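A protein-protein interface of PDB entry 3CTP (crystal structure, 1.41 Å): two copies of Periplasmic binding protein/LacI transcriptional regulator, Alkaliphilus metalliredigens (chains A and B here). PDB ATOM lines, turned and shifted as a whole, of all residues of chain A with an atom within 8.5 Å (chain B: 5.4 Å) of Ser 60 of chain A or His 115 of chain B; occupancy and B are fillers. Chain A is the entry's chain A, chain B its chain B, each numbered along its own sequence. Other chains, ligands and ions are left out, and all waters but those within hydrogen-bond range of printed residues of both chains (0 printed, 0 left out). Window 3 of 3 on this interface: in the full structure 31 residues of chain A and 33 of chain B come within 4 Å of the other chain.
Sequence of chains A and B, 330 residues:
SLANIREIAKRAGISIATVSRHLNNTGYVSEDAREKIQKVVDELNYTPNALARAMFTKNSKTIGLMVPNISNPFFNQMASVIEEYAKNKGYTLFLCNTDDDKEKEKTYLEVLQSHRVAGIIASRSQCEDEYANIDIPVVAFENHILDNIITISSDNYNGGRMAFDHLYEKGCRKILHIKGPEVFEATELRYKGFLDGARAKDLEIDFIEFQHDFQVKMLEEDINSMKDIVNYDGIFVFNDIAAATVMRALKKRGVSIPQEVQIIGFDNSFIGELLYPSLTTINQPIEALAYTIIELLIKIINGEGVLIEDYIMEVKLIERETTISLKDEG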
ATOM      1  N   SER A  60     -21.355  21.606  -3.530  1.00  0.00           N
ATOM      2  CA  SER A  60     -21.284  20.639  -4.656  1.00  0.00           C
ATOM      3  C   SER A  60     -22.631  20.531  -5.369  1.00  0.00           C
ATOM      4  O   SER A  60     -23.685  20.444  -4.733  1.00  0.00           O
ATOM      5  CB  SER A  60     -20.897  19.252  -4.133  1.00  0.00           C
ATOM      6  OG  SER A  60     -21.014  18.285  -5.160  1.00  0.00           O
ATOM      7  N   LYS A  61     -22.598  20.524  -6.693  1.00  0.00           N
ATOM      8  CA  LYS A  61     -23.788  20.166  -7.428  1.00  0.00           C
ATOM      9  C   LYS A  61     -23.556  18.840  -8.106  1.00  0.00           C
ATOM     10  O   LYS A  61     -23.983  18.648  -9.231  1.00  0.00           O
ATOM     11  CB  LYS A  61     -24.158  21.244  -8.454  1.00  0.00           C
ATOM     12  CG  LYS A  61     -24.451  22.587  -7.803  1.00  0.00           C
ATOM     13  CD  LYS A  61     -25.699  22.482  -6.935  1.00  0.00           C
ATOM     14  CE  LYS A  61     -26.981  22.534  -7.772  1.00  0.00           C
ATOM     15  NZ  LYS A  61     -28.141  22.896  -6.901  1.00  0.00           N
ATOM     16  N   THR A  62     -22.925  17.902  -7.394  1.00  0.00           N
ATOM     17  CA  THR A  62     -22.712  16.567  -7.943  1.00  0.00           C
ATOM     18  C   THR A  62     -23.303  15.512  -7.014  1.00  0.00           C
ATOM     19  O   THR A  62     -23.213  15.642  -5.775  1.00  0.00           O
ATOM     20  CB  THR A  62     -21.233  16.296  -8.203  1.00  0.00           C
ATOM     21  OG1 THR A  62     -20.751  17.280  -9.138  1.00  0.00           O
ATOM     22  CG2 THR A  62     -21.022  14.904  -8.820  1.00  0.00           C
ATOM     23  N   ILE A  63     -23.931  14.514  -7.625  1.00  0.00           N
ATOM     24  CA  ILE A  63     -24.500  13.367  -6.911  1.00  0.00           C
ATOM     25  C   ILE A  63     -23.673  12.137  -7.274  1.00  0.00           C
ATOM     26  O   ILE A  63     -23.246  11.986  -8.425  1.00  0.00           O
ATOM     27  CB  ILE A  63     -25.942  13.143  -7.364  1.00  0.00           C
ATOM     28  CG1 ILE A  63     -26.794  14.246  -6.756  1.00  0.00           C
ATOM     29  CG2 ILE A  63     -26.433  11.744  -6.956  1.00  0.00           C
ATOM     30  CD1 ILE A  63     -28.137  14.489  -7.477  1.00  0.00           C
ATOM     31  N   GLY A  64     -23.407  11.274  -6.303  1.00  0.00           N
ATOM     32  CA  GLY A  64     -22.680  10.036  -6.605  1.00  0.00           C
ATOM     33  C   GLY A  64     -23.679   8.928  -6.822  1.00  0.00           C
ATOM     34  O   GLY A  64     -24.571   8.732  -5.988  1.00  0.00           O
ATOM     35  N   GLY A  90     -30.279  20.424 -11.874  1.00  0.00           N
ATOM     36  CA  GLY A  90     -29.032  21.163 -11.754  1.00  0.00           C
ATOM     37  C   GLY A  90     -27.824  20.405 -11.215  1.00  0.00           C
ATOM     38  O   GLY A  90     -26.854  21.045 -10.796  1.00  0.00           O
ATOM     39  N   TYR A  91     -27.844  19.067 -11.290  1.00  0.00           N
ATOM     40  CA  TYR A  91     -26.745  18.248 -10.754  1.00  0.00           C
ATOM     41  C   TYR A  91     -26.053  17.439 -11.845  1.00  0.00           C
ATOM     42  O   TYR A  91     -26.694  16.998 -12.814  1.00  0.00           O
ATOM     43  CB  TYR A  91     -27.282  17.256  -9.709  1.00  0.00           C
ATOM     44  CG  TYR A  91     -27.753  17.938  -8.455  1.00  0.00           C
ATOM     45  CD1 TYR A  91     -26.910  18.068  -7.363  1.00  0.00           C
ATOM     46  CD2 TYR A  91     -29.032  18.490  -8.382  1.00  0.00           C
ATOM     47  CE1 TYR A  91     -27.339  18.692  -6.206  1.00  0.00           C
ATOM     48  CE2 TYR A  91     -29.456  19.136  -7.252  1.00  0.00           C
ATOM     49  CZ  TYR A  91     -28.614  19.249  -6.165  1.00  0.00           C
ATOM     50  OH  TYR A  91     -29.074  19.906  -5.032  1.00  0.00           O
ATOM     51  N   THR A  92     -24.743  17.251 -11.677  1.00  0.00           N
ATOM     52  CA  THR A  92     -24.008  16.265 -12.474  1.00  0.00           C
ATOM     53  C   THR A  92     -23.858  14.975 -11.658  1.00  0.00           C
ATOM     54  O   THR A  92     -24.183  14.957 -10.477  1.00  0.00           O
ATOM     55  CB  THR A  92     -22.647  16.798 -12.837  1.00  0.00           C
ATOM     56  OG1 THR A  92     -22.062  17.416 -11.691  1.00  0.00           O
ATOM     57  CG2 THR A  92     -22.813  17.903 -13.884  1.00  0.00           C
ATOM     58  N   PHE A  94     -21.313  11.484 -10.639  1.00  0.00           N
ATOM     59  CA  PHE A  94     -20.132  10.614 -10.686  1.00  0.00           C
ATOM     60  C   PHE A  94     -20.659   9.192 -10.584  1.00  0.00           C
ATOM     61  O   PHE A  94     -21.435   8.896  -9.667  1.00  0.00           O
ATOM     62  CB  PHE A  94     -19.225  10.848  -9.479  1.00  0.00           C
ATOM     63  CG  PHE A  94     -18.442  12.134  -9.516  1.00  0.00           C
ATOM     64  CD1 PHE A  94     -18.039  12.676 -10.709  1.00  0.00           C
ATOM     65  CD2 PHE A  94     -18.065  12.744  -8.342  1.00  0.00           C
ATOM     66  CE1 PHE A  94     -17.285  13.868 -10.741  1.00  0.00           C
ATOM     67  CE2 PHE A  94     -17.322  13.900  -8.361  1.00  0.00           C
ATOM     68  CZ  PHE A  94     -16.948  14.469  -9.548  1.00  0.00           C
ATOM     69  N   VAL A 111     -15.004   7.732  -0.251  1.00  0.00           N
ATOM     70  CA  VAL A 111     -14.480   8.639  -1.261  1.00  0.00           C
ATOM     71  C   VAL A 111     -15.531   9.706  -1.616  1.00  0.00           C
ATOM     72  O   VAL A 111     -15.215  10.900  -1.711  1.00  0.00           O
ATOM     73  CB  VAL A 111     -14.056   7.865  -2.505  1.00  0.00           C
ATOM     74  CG1 VAL A 111     -13.655   8.824  -3.600  1.00  0.00           C
ATOM     75  CG2 VAL A 111     -12.899   6.920  -2.158  1.00  0.00           C
ATOM     76  N   LEU A 112     -16.785   9.300  -1.803  1.00  0.00           N
ATOM     77  CA  LEU A 112     -17.838  10.285  -2.084  1.00  0.00           C
ATOM     78  C   LEU A 112     -17.996  11.287  -0.941  1.00  0.00           C
ATOM     79  O   LEU A 112     -18.163  12.485  -1.168  1.00  0.00           O
ATOM     80  CB  LEU A 112     -19.165   9.562  -2.354  1.00  0.00           C
ATOM     81  CG  LEU A 112     -19.158   8.796  -3.681  1.00  0.00           C
ATOM     82  CD1 LEU A 112     -20.313   7.796  -3.784  1.00  0.00           C
ATOM     83  CD2 LEU A 112     -19.179   9.809  -4.870  1.00  0.00           C
ATOM     84  N   GLN A 113     -17.965  10.809   0.299  1.00  0.00           N
ATOM     85  CA  GLN A 113     -18.028  11.719   1.460  1.00  0.00           C
ATOM     86  C   GLN A 113     -16.855  12.699   1.476  1.00  0.00           C
ATOM     87  O   GLN A 113     -17.025  13.893   1.764  1.00  0.00           O
ATOM     88  CB  GLN A 113     -18.035  10.899   2.758  1.00  0.00           C
ATOM     89  CG  GLN A 113     -17.729  11.678   4.018  1.00  0.00           C
ATOM     90  CD  GLN A 113     -17.765  10.788   5.248  1.00  0.00           C
ATOM     91  OE1 GLN A 113     -16.720  10.399   5.775  1.00  0.00           O
ATOM     92  NE2 GLN A 113     -18.967  10.436   5.691  1.00  0.00           N
ATOM     93  N   SER A 114     -15.653  12.201   1.185  1.00  0.00           N
ATOM     94  CA  SER A 114     -14.463  13.039   1.252  1.00  0.00           C
ATOM     95  C   SER A 114     -14.511  14.107   0.166  1.00  0.00           C
ATOM     96  O   SER A 114     -13.966  15.205   0.324  1.00  0.00           O
ATOM     97  CB  SER A 114     -13.190  12.189   1.129  1.00  0.00           C
ATOM     98  OG  SER A 114     -12.962  11.801  -0.221  1.00  0.00           O
ATOM     99  N   HIS A 115     -15.201  13.792  -0.933  1.00  0.00           N
ATOM    100  CA  HIS A 115     -15.402  14.748  -2.039  1.00  0.00           C
ATOM    101  C   HIS A 115     -16.644  15.621  -1.888  1.00  0.00           C
ATOM    102  O   HIS A 115     -16.951  16.432  -2.769  1.00  0.00           O
ATOM    103  CB  HIS A 115     -15.437  14.007  -3.377  1.00  0.00           C
ATOM    104  CG  HIS A 115     -14.082  13.611  -3.849  1.00  0.00           C
ATOM    105  ND1 HIS A 115     -13.433  12.488  -3.379  1.00  0.00           N
ATOM    106  CD2 HIS A 115     -13.216  14.221  -4.694  1.00  0.00           C
ATOM    107  CE1 HIS A 115     -12.240  12.407  -3.937  1.00  0.00           C
ATOM    108  NE2 HIS A 115     -12.082  13.448  -4.735  1.00  0.00           N
ATOM    109  N   ARG A 116     -17.356  15.456  -0.782  1.00  0.00           N
ATOM    110  CA  ARG A 116     -18.456  16.340  -0.431  1.00  0.00           C
ATOM    111  C   ARG A 116     -19.520  16.418  -1.520  1.00  0.00           C
ATOM    112  O   ARG A 116     -20.007  17.513  -1.859  1.00  0.00           O
ATOM    113  CB  ARG A 116     -17.941  17.756  -0.129  1.00  0.00           C
ATOM    114  CG  ARG A 116     -17.101  17.857   1.135  1.00  0.00           C
ATOM    115  CD  ARG A 116     -16.745  19.323   1.392  1.00  0.00           C
ATOM    116  NE  ARG A 116     -16.385  19.573   2.783  1.00  0.00           N
ATOM    117  CZ  ARG A 116     -17.249  19.930   3.728  1.00  0.00           C
ATOM    118  NH1 ARG A 116     -18.539  20.067   3.434  1.00  0.00           N
ATOM    119  NH2 ARG A 116     -16.828  20.132   4.968  1.00  0.00           N
ATOM    120  N   VAL A 117     -19.878  15.278  -2.086  1.00  0.00           N
ATOM    121  CA  VAL A 117     -21.008  15.282  -3.033  1.00  0.00           C
ATOM    122  C   VAL A 117     -22.284  15.691  -2.318  1.00  0.00           C
ATOM    123  O   VAL A 117     -22.388  15.583  -1.088  1.00  0.00           O
ATOM    124  CB  VAL A 117     -21.177  13.918  -3.743  1.00  0.00           C
ATOM    125  CG1 VAL A 117     -19.907  13.598  -4.524  1.00  0.00           C
ATOM    126  CG2 VAL A 117     -21.511  12.805  -2.736  1.00  0.00           C
ATOM    127  N   ALA A 118     -23.286  16.133  -3.080  1.00  0.00           N
ATOM    128  CA  ALA A 118     -24.498  16.634  -2.478  1.00  0.00           C
ATOM    129  C   ALA A 118     -25.384  15.509  -1.979  1.00  0.00           C
ATOM    130  O   ALA A 118     -26.189  15.695  -1.068  1.00  0.00           O
ATOM    131  CB  ALA A 118     -25.284  17.472  -3.498  1.00  0.00           C
ATOM    132  N   GLY A 119     -25.267  14.351  -2.618  1.00  0.00           N
ATOM    133  CA  GLY A 119     -26.121  13.216  -2.264  1.00  0.00           C
ATOM    134  C   GLY A 119     -25.583  11.955  -2.921  1.00  0.00           C
ATOM    135  O   GLY A 119     -24.746  12.034  -3.803  1.00  0.00           O
ATOM    136  N   ILE A 301     -31.974  16.357   0.124  1.00  0.00           N
ATOM    137  CA  ILE A 301     -30.933  17.381   0.054  1.00  0.00           C
ATOM    138  C   ILE A 301     -31.433  18.728   0.550  1.00  0.00           C
ATOM    139  O   ILE A 301     -30.714  19.453   1.260  1.00  0.00           O
ATOM    140  CB  ILE A 301     -30.399  17.528  -1.396  1.00  0.00           C
ATOM    141  CG1 ILE A 301     -29.591  16.286  -1.785  1.00  0.00           C
ATOM    142  CG2 ILE A 301     -29.599  18.855  -1.549  1.00  0.00           C
ATOM    143  CD1 ILE A 301     -29.255  16.254  -3.297  1.00  0.00           C
ATOM    144  N   SER B  60      -6.114  14.200  -3.459  1.00  0.00           N
ATOM    145  CA  SER B  60      -6.981  13.000  -3.385  1.00  0.00           C
ATOM    146  C   SER B  60      -6.324  11.834  -4.117  1.00  0.00           C
ATOM    147  O   SER B  60      -5.370  12.002  -4.871  1.00  0.00           O
ATOM    148  CB  SER B  60      -8.327  13.282  -4.035  1.00  0.00           C
ATOM    149  OG  SER B  60      -8.234  13.072  -5.438  1.00  0.00           O
ATOM    150  N   GLU B 110     -14.735  20.563 -15.882  1.00  0.00           N
ATOM    151  CA  GLU B 110     -14.836  21.584 -14.838  1.00  0.00           C
ATOM    152  C   GLU B 110     -15.147  20.967 -13.462  1.00  0.00           C
ATOM    153  O   GLU B 110     -14.604  21.374 -12.413  1.00  0.00           O
ATOM    154  CB  GLU B 110     -15.913  22.616 -15.221  1.00  0.00           C
ATOM    155  CG  GLU B 110     -15.559  23.368 -16.502  1.00  0.00           C
ATOM    156  CD  GLU B 110     -16.617  24.381 -16.901  1.00  0.00           C
ATOM    157  OE1 GLU B 110     -17.533  24.641 -16.085  1.00  0.00           O
ATOM    158  OE2 GLU B 110     -16.527  24.919 -18.024  1.00  0.00           O
ATOM    159  N   VAL B 111     -16.035  19.993 -13.469  1.00  0.00           N
ATOM    160  CA  VAL B 111     -16.427  19.353 -12.232  1.00  0.00           C
ATOM    161  C   VAL B 111     -15.249  18.577 -11.646  1.00  0.00           C
ATOM    162  O   VAL B 111     -14.994  18.629 -10.439  1.00  0.00           O
ATOM    163  CB  VAL B 111     -17.608  18.432 -12.472  1.00  0.00           C
ATOM    164  CG1 VAL B 111     -17.851  17.569 -11.231  1.00  0.00           C
ATOM    165  CG2 VAL B 111     -18.837  19.265 -12.794  1.00  0.00           C
ATOM    166  N   LEU B 112     -14.518  17.859 -12.493  1.00  0.00           N
ATOM    167  CA  LEU B 112     -13.352  17.114 -11.992  1.00  0.00           C
ATOM    168  C   LEU B 112     -12.284  18.060 -11.455  1.00  0.00           C
ATOM    169  O   LEU B 112     -11.618  17.755 -10.454  1.00  0.00           O
ATOM    170  CB  LEU B 112     -12.777  16.226 -13.104  1.00  0.00           C
ATOM    171  CG  LEU B 112     -13.718  15.083 -13.446  1.00  0.00           C
ATOM    172  CD1 LEU B 112     -13.358  14.451 -14.789  1.00  0.00           C
ATOM    173  CD2 LEU B 112     -13.704  14.014 -12.315  1.00  0.00           C
ATOM    174  N   GLN B 113     -12.094  19.208 -12.105  1.00  0.00           N
ATOM    175  CA  GLN B 113     -11.108  20.185 -11.608  1.00  0.00           C
ATOM    176  C   GLN B 113     -11.546  20.754 -10.274  1.00  0.00           C
ATOM    177  O   GLN B 113     -10.725  20.968  -9.375  1.00  0.00           O
ATOM    178  CB  GLN B 113     -10.918  21.330 -12.602  1.00  0.00           C
ATOM    179  CG  GLN B 113     -10.141  20.914 -13.837  1.00  0.00           C
ATOM    180  CD  GLN B 113      -9.986  22.040 -14.841  1.00  0.00           C
ATOM    181  OE1 GLN B 113      -9.485  23.125 -14.517  1.00  0.00           O
ATOM    182  NE2 GLN B 113     -10.410  21.787 -16.072  1.00  0.00           N
ATOM    183  N   SER B 114     -12.842  21.020 -10.143  1.00  0.00           N
ATOM    184  CA  SER B 114     -13.358  21.612  -8.900  1.00  0.00           C
ATOM    185  C   SER B 114     -13.201  20.662  -7.738  1.00  0.00           C
ATOM    186  O   SER B 114     -13.046  21.091  -6.586  1.00  0.00           O
ATOM    187  CB  SER B 114     -14.827  21.964  -9.041  1.00  0.00           C
ATOM    188  OG  SER B 114     -14.965  23.101  -9.879  1.00  0.00           O
ATOM    189  N   HIS B 115     -13.254  19.369  -8.049  1.00  0.00           N
ATOM    190  CA  HIS B 115     -13.060  18.303  -7.052  1.00  0.00           C
ATOM    191  C   HIS B 115     -11.602  17.906  -6.851  1.00  0.00           C
ATOM    192  O   HIS B 115     -11.305  17.019  -6.046  1.00  0.00           O
ATOM    193  CB  HIS B 115     -13.898  17.084  -7.435  1.00  0.00           C
ATOM    194  CG  HIS B 115     -15.340  17.248  -7.097  1.00  0.00           C
ATOM    195  ND1 HIS B 115     -16.227  17.921  -7.912  1.00  0.00           N
ATOM    196  CD2 HIS B 115     -16.034  16.905  -5.987  1.00  0.00           C
ATOM    197  CE1 HIS B 115     -17.410  17.959  -7.327  1.00  0.00           C
ATOM    198  NE2 HIS B 115     -17.319  17.346  -6.161  1.00  0.00           N
ATOM    199  N   ARG B 116     -10.697  18.536  -7.582  1.00  0.00           N
ATOM    200  CA  ARG B 116      -9.269  18.347  -7.359  1.00  0.00           C
ATOM    201  C   ARG B 116      -8.877  16.876  -7.464  1.00  0.00           C
ATOM    202  O   ARG B 116      -8.091  16.358  -6.649  1.00  0.00           O
ATOM    203  CB  ARG B 116      -8.907  18.859  -5.968  1.00  0.00           C
ATOM    204  CG  ARG B 116      -9.472  20.231  -5.729  1.00  0.00           C
ATOM    205  CD  ARG B 116      -8.838  21.176  -6.693  1.00  0.00           C
ATOM    206  NE  ARG B 116      -7.483  21.501  -6.259  1.00  0.00           N
ATOM    207  CZ  ARG B 116      -7.025  21.234  -5.042  1.00  0.00           C
ATOM    208  NH1 ARG B 116      -7.825  20.654  -4.159  1.00  0.00           N
ATOM    209  NH2 ARG B 116      -5.778  21.551  -4.700  1.00  0.00           N
ATOM    210  N   VAL B 117      -9.407  16.187  -8.457  1.00  0.00           N
ATOM    211  CA  VAL B 117      -8.926  14.819  -8.694  1.00  0.00           C
ATOM    212  C   VAL B 117      -7.445  14.808  -9.040  1.00  0.00           C
ATOM    213  O   VAL B 117      -6.857  15.818  -9.459  1.00  0.00           O
ATOM    214  CB  VAL B 117      -9.722  14.102  -9.794  1.00  0.00           C
ATOM    215  CG1 VAL B 117     -11.209  14.018  -9.394  1.00  0.00           C
ATOM    216  CG2 VAL B 117      -9.541  14.804 -11.147  1.00  0.00           C
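The backbone carbonyl oxygen (O) of Thr 92 of chain A sits at hydrogen-bond distance from the backbone NH (N) of Ile 63 of chain A (2.9 Å). The backbone carbonyl oxygen (O) of Val 111 of chain B is in hydrogen-bond range of a ring nitrogen (ND1) of His 115 of chain B. The side-chain hydroxyl (OG1) of Thr 92 of chain A lies within hydrogen-bond range of the side-chain hydroxyl (OG1) of Thr 62 of chain A (2.9 Å). The side-chain hydroxyl (OG) of Ser 60 of chain A is in hydrogen-bond range of the backbone NH (N) of Thr 62 of chain A (3.0 Å). The backbone carbonyl oxygen (O) of Leu 112 of chain B is in hydrogen-bond range of the backbone NH (N) of Val 117 of chain B (3.4 Å). O of Thr 62 of chain A is in hydrogen-bond range of N of Ala 118 of chain A.
Among the printed residues, merely in contact across the chains: His 115 of chain A with His 115 of chain B, Thr 62 of chain A with Val 111 of chain B, Phe 94 of chain A with Val 111 of chain B, His 115 of chain A with Ser 60 of chain B, Thr 62 of chain A with His 115 of chain B, Thr 92 of chain A with Val 111 of chain B, Phe 94 of chain A with His 115 of chain B, Phe 94 of chain A with Leu 112 of chain B and Ser 60 of chain A with His 115 of chain B.
Of chain B, only His 115 (3.9 Å) comes within 4 Å of Ser 60 of chain A. Printed residues of chain A within 4 Å of His 115 of chain B: Ser 60 (3.9 Å), Thr 62 (3.9 Å), Phe 94 (3.9 Å) and His 115 (3.4 Å). Of the printed residues of chain B, Phe 94 of chain A touches Val 111, Leu 112 and His 115. Printed residues of chain A within 4 Å of Leu 112 of chain B: Phe 94 (3.9 Å). Of the printed residues of chain B, Thr 62 of chain A touches Val 111 and His 115. Of the printed residues of chain B, Thr 92 of chain A touches Val 111 (3.9 Å). Of the printed residues of chain A, Ser 60 of chain B touches His 115. Gly 119 of chain A touches none of the printed residues of chain B. The nearest printed residue of chain B that does not touch Ser 60 of chain A is Val 111 of chain B (6.9 Å). The nearest residue of chain A that does not touch His 115 of chain B is Val 117 of chain A (4.8 Å).
Of the 9 printed residues of chain B, 4 touch a printed residue of chain A. Hydrophobic or aromatic side chains of chain B that line the printed part of chain A: Val 111, Leu 112 and His 115.
Ser 60 of chain A touches His 115 of chain B, and with the chains exchanged His 115 of chain A touches Ser 60 of chain B. His 115 of chain A touches its own counterpart, His 115 of chain B. 8 positions are printed for both chains.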
